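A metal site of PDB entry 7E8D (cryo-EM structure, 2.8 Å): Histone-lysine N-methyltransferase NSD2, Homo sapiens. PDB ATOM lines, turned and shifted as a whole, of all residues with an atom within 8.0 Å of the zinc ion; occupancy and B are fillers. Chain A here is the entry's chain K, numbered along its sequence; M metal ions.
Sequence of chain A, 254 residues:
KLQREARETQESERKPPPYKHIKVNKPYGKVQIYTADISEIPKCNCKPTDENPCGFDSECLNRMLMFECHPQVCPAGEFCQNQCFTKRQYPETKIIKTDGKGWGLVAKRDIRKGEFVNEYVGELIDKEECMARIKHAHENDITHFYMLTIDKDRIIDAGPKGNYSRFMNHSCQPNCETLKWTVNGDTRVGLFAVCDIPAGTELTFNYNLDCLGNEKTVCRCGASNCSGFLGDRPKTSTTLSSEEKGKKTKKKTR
The side-chain sulfur of Cys 221 sits close to the backbone NH of Ala 223.
SG of Cys 172 sits close to N of Ser 227.
The side-chain sulfur of Cys 226 lies close to the backbone NH of Gly 228.
The backbone NH (N) of Cys 219 is in hydrogen-bond range of the backbone carbonyl oxygen (O) of Gly 228 (2.5 Å).
The side-chain sulfur (SG) of Cys 172 lies close to a ring nitrogen (NE2) of His 170, at 3.7 Å.
Ser 227 touches the zinc ion (N to ZN, 3.97 Å).
The nearest printed residue that does not touch the zinc ion is Gly 228 (4.5 Å).
The zinc ion is bound by the side-chain sulfur (SG) of Cys 221 (2.3 Å).
The zinc ion is bound by SG of Cys 172 (2.3 Å).
SG of Cys 219 is bound to the zinc ion (2.3 Å).
The zinc ion is bound by SG of Cys 226, at 2.3 Å.
The zinc ion has four donor atoms within binding distance.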
ATOM      1  N   HIS A 170      28.476 -11.327 -12.335  1.00  0.00           N
ATOM      2  CA  HIS A 170      28.432 -12.380 -11.336  1.00  0.00           C
ATOM      3  C   HIS A 170      28.085 -13.714 -11.989  1.00  0.00           C
ATOM      4  O   HIS A 170      27.234 -13.784 -12.878  1.00  0.00           O
ATOM      5  CB  HIS A 170      27.404 -12.055 -10.262  1.00  0.00           C
ATOM      6  CG  HIS A 170      26.985 -13.259  -9.476  1.00  0.00           C
ATOM      7  ND1 HIS A 170      27.885 -14.045  -8.806  1.00  0.00           N
ATOM      8  CD2 HIS A 170      25.772 -13.816  -9.281  1.00  0.00           C
ATOM      9  CE1 HIS A 170      27.239 -15.033  -8.206  1.00  0.00           C
ATOM     10  NE2 HIS A 170      25.955 -14.922  -8.481  1.00  0.00           N
ATOM     11  N   SER A 171      28.756 -14.763 -11.550  1.00  0.00           N
ATOM     12  CA  SER A 171      28.393 -16.114 -11.940  1.00  0.00           C
ATOM     13  C   SER A 171      28.580 -17.033 -10.745  1.00  0.00           C
ATOM     14  O   SER A 171      29.628 -17.003 -10.096  1.00  0.00           O
ATOM     15  CB  SER A 171      29.241 -16.607 -13.113  1.00  0.00           C
ATOM     16  OG  SER A 171      30.348 -17.342 -12.635  1.00  0.00           O
ATOM     17  N   CYS A 172      27.574 -17.867 -10.485  1.00  0.00           N
ATOM     18  CA  CYS A 172      27.608 -18.717  -9.305  1.00  0.00           C
ATOM     19  C   CYS A 172      28.764 -19.697  -9.332  1.00  0.00           C
ATOM     20  O   CYS A 172      29.167 -20.190  -8.277  1.00  0.00           O
ATOM     21  CB  CYS A 172      26.284 -19.467  -9.174  1.00  0.00           C
ATOM     22  SG  CYS A 172      24.828 -18.395  -9.036  1.00  0.00           S
ATOM     23  N   GLN A 173      29.313 -19.976 -10.504  1.00  0.00           N
ATOM     24  CA  GLN A 173      30.511 -20.802 -10.644  1.00  0.00           C
ATOM     25  C   GLN A 173      31.503 -19.959 -11.444  1.00  0.00           C
ATOM     26  O   GLN A 173      31.580 -20.075 -12.681  1.00  0.00           O
ATOM     27  CB  GLN A 173      30.197 -22.132 -11.322  1.00  0.00           C
ATOM     28  CG  GLN A 173      31.253 -23.203 -11.105  1.00  0.00           C
ATOM     29  CD  GLN A 173      32.303 -23.197 -12.180  1.00  0.00           C
ATOM     30  OE1 GLN A 173      32.080 -22.705 -13.279  1.00  0.00           O
ATOM     31  NE2 GLN A 173      33.464 -23.768 -11.870  1.00  0.00           N
ATOM     32  N   VAL A 218      17.064 -11.525 -10.229  1.00  0.00           N
ATOM     33  CA  VAL A 218      17.348 -12.877 -10.696  1.00  0.00           C
ATOM     34  C   VAL A 218      18.761 -12.970 -11.234  1.00  0.00           C
ATOM     35  O   VAL A 218      19.291 -12.015 -11.827  1.00  0.00           O
ATOM     36  CB  VAL A 218      16.315 -13.309 -11.760  1.00  0.00           C
ATOM     37  CG1 VAL A 218      16.422 -12.430 -12.991  1.00  0.00           C
ATOM     38  CG2 VAL A 218      16.486 -14.773 -12.123  1.00  0.00           C
ATOM     39  N   CYS A 219      19.401 -14.112 -11.017  1.00  0.00           N
ATOM     40  CA  CYS A 219      20.761 -14.362 -11.478  1.00  0.00           C
ATOM     41  C   CYS A 219      20.673 -15.241 -12.723  1.00  0.00           C
ATOM     42  O   CYS A 219      20.546 -16.461 -12.622  1.00  0.00           O
ATOM     43  CB  CYS A 219      21.587 -15.042 -10.386  1.00  0.00           C
ATOM     44  SG  CYS A 219      23.155 -15.691 -10.990  1.00  0.00           S
ATOM     45  N   ARG A 220      20.749 -14.601 -13.884  1.00  0.00           N
ATOM     46  CA  ARG A 220      20.801 -15.328 -15.156  1.00  0.00           C
ATOM     47  C   ARG A 220      22.235 -15.653 -15.539  1.00  0.00           C
ATOM     48  O   ARG A 220      22.676 -15.402 -16.669  1.00  0.00           O
ATOM     49  CB  ARG A 220      20.097 -14.521 -16.238  1.00  0.00           C
ATOM     50  N   CYS A 221      22.988 -16.215 -14.604  1.00  0.00           N
ATOM     51  CA  CYS A 221      24.402 -16.486 -14.847  1.00  0.00           C
ATOM     52  C   CYS A 221      24.581 -17.659 -15.804  1.00  0.00           C
ATOM     53  O   CYS A 221      25.371 -17.588 -16.748  1.00  0.00           O
ATOM     54  CB  CYS A 221      25.122 -16.760 -13.537  1.00  0.00           C
ATOM     55  SG  CYS A 221      24.920 -18.425 -12.899  1.00  0.00           S
ATOM     56  N   GLY A 222      23.847 -18.757 -15.581  1.00  0.00           N
ATOM     57  CA  GLY A 222      23.994 -19.943 -16.393  1.00  0.00           C
ATOM     58  C   GLY A 222      24.880 -21.017 -15.808  1.00  0.00           C
ATOM     59  O   GLY A 222      25.181 -21.984 -16.505  1.00  0.00           O
ATOM     60  N   ALA A 223      25.319 -20.874 -14.563  1.00  0.00           N
ATOM     61  CA  ALA A 223      26.132 -21.904 -13.936  1.00  0.00           C
ATOM     62  C   ALA A 223      25.297 -23.138 -13.626  1.00  0.00           C
ATOM     63  O   ALA A 223      24.080 -23.053 -13.447  1.00  0.00           O
ATOM     64  CB  ALA A 223      26.788 -21.378 -12.671  1.00  0.00           C
ATOM     65  N   SER A 224      25.973 -24.286 -13.549  1.00  0.00           N
ATOM     66  CA  SER A 224      25.276 -25.521 -13.200  1.00  0.00           C
ATOM     67  C   SER A 224      24.682 -25.440 -11.800  1.00  0.00           C
ATOM     68  O   SER A 224      23.551 -25.878 -11.576  1.00  0.00           O
ATOM     69  CB  SER A 224      26.241 -26.699 -13.310  1.00  0.00           C
ATOM     70  OG  SER A 224      26.821 -26.766 -14.603  1.00  0.00           O
ATOM     71  N   ASN A 225      25.431 -24.876 -10.851  1.00  0.00           N
ATOM     72  CA  ASN A 225      24.957 -24.703  -9.483  1.00  0.00           C
ATOM     73  C   ASN A 225      24.383 -23.309  -9.252  1.00  0.00           C
ATOM     74  O   ASN A 225      24.500 -22.762  -8.148  1.00  0.00           O
ATOM     75  CB  ASN A 225      26.080 -24.997  -8.485  1.00  0.00           C
ATOM     76  CG  ASN A 225      25.578 -25.106  -7.055  1.00  0.00           C
ATOM     77  OD1 ASN A 225      24.385 -25.277  -6.810  1.00  0.00           O
ATOM     78  ND2 ASN A 225      26.491 -24.989  -6.102  1.00  0.00           N
ATOM     79  N   CYS A 226      23.778 -22.704 -10.272  1.00  0.00           N
ATOM     80  CA  CYS A 226      23.267 -21.357 -10.119  1.00  0.00           C
ATOM     81  C   CYS A 226      22.216 -21.323  -9.019  1.00  0.00           C
ATOM     82  O   CYS A 226      21.316 -22.152  -8.971  1.00  0.00           O
ATOM     83  CB  CYS A 226      22.662 -20.853 -11.427  1.00  0.00           C
ATOM     84  SG  CYS A 226      21.775 -19.293 -11.232  1.00  0.00           S
ATOM     85  N   SER A 227      22.347 -20.343  -8.122  1.00  0.00           N
ATOM     86  CA  SER A 227      21.397 -20.144  -7.043  1.00  0.00           C
ATOM     87  C   SER A 227      20.162 -19.388  -7.500  1.00  0.00           C
ATOM     88  O   SER A 227      19.392 -18.920  -6.655  1.00  0.00           O
ATOM     89  CB  SER A 227      22.058 -19.408  -5.883  1.00  0.00           C
ATOM     90  OG  SER A 227      23.044 -20.203  -5.258  1.00  0.00           O
ATOM     91  N   GLY A 228      19.957 -19.249  -8.800  1.00  0.00           N
ATOM     92  CA  GLY A 228      18.766 -18.605  -9.321  1.00  0.00           C
ATOM     93  C   GLY A 228      18.777 -17.106  -9.145  1.00  0.00           C
ATOM     94  O   GLY A 228      18.654 -16.352 -10.110  1.00  0.00           O
ATOM     95  N   PHE A 229      18.900 -16.659  -7.902  1.00  0.00           N
ATOM     96  CA  PHE A 229      19.001 -15.242  -7.579  1.00  0.00           C
ATOM     97  C   PHE A 229      20.441 -14.930  -7.153  1.00  0.00           C
ATOM     98  O   PHE A 229      21.319 -15.778  -7.186  1.00  0.00           O
ATOM     99  CB  PHE A 229      18.006 -14.871  -6.490  1.00  0.00           C
ATOM    100  CG  PHE A 229      16.586 -14.765  -6.987  1.00  0.00           C
ATOM    101  CD1 PHE A 229      16.264 -15.092  -8.287  1.00  0.00           C
ATOM    102  CD2 PHE A 229      15.583 -14.334  -6.144  1.00  0.00           C
ATOM    103  CE1 PHE A 229      14.970 -15.001  -8.740  1.00  0.00           C
ATOM    104  CE2 PHE A 229      14.285 -14.220  -6.589  1.00  0.00           C
ATOM    105  CZ  PHE A 229      13.972 -14.557  -7.893  1.00  0.00           C
ATOM    106  N   LEU A 230      20.647 -13.677  -6.751  1.00  0.00           N
ATOM    107  CA  LEU A 230      21.973 -13.232  -6.307  1.00  0.00           C
ATOM    108  C   LEU A 230      22.131 -13.563  -4.832  1.00  0.00           C
ATOM    109  O   LEU A 230      22.050 -12.703  -3.943  1.00  0.00           O
ATOM    110  CB  LEU A 230      22.154 -11.744  -6.590  1.00  0.00           C
ATOM    111  CG  LEU A 230      21.940 -11.338  -8.048  1.00  0.00           C
ATOM    112  CD1 LEU A 230      22.028  -9.835  -8.214  1.00  0.00           C
ATOM    113  CD2 LEU A 230      22.946 -12.018  -8.937  1.00  0.00           C
ATOM    114  N   GLY A 231      22.366 -14.841  -4.552  1.00  0.00           N
ATOM    115  CA  GLY A 231      22.542 -15.318  -3.191  1.00  0.00           C
ATOM    116  C   GLY A 231      22.421 -16.817  -3.053  1.00  0.00           C
ATOM    117  O   GLY A 231      23.371 -17.510  -2.684  1.00  0.00           O
HETATM  118 ZN    ZN M   1      23.670 -17.959 -11.002  1.00  0.00          ZN
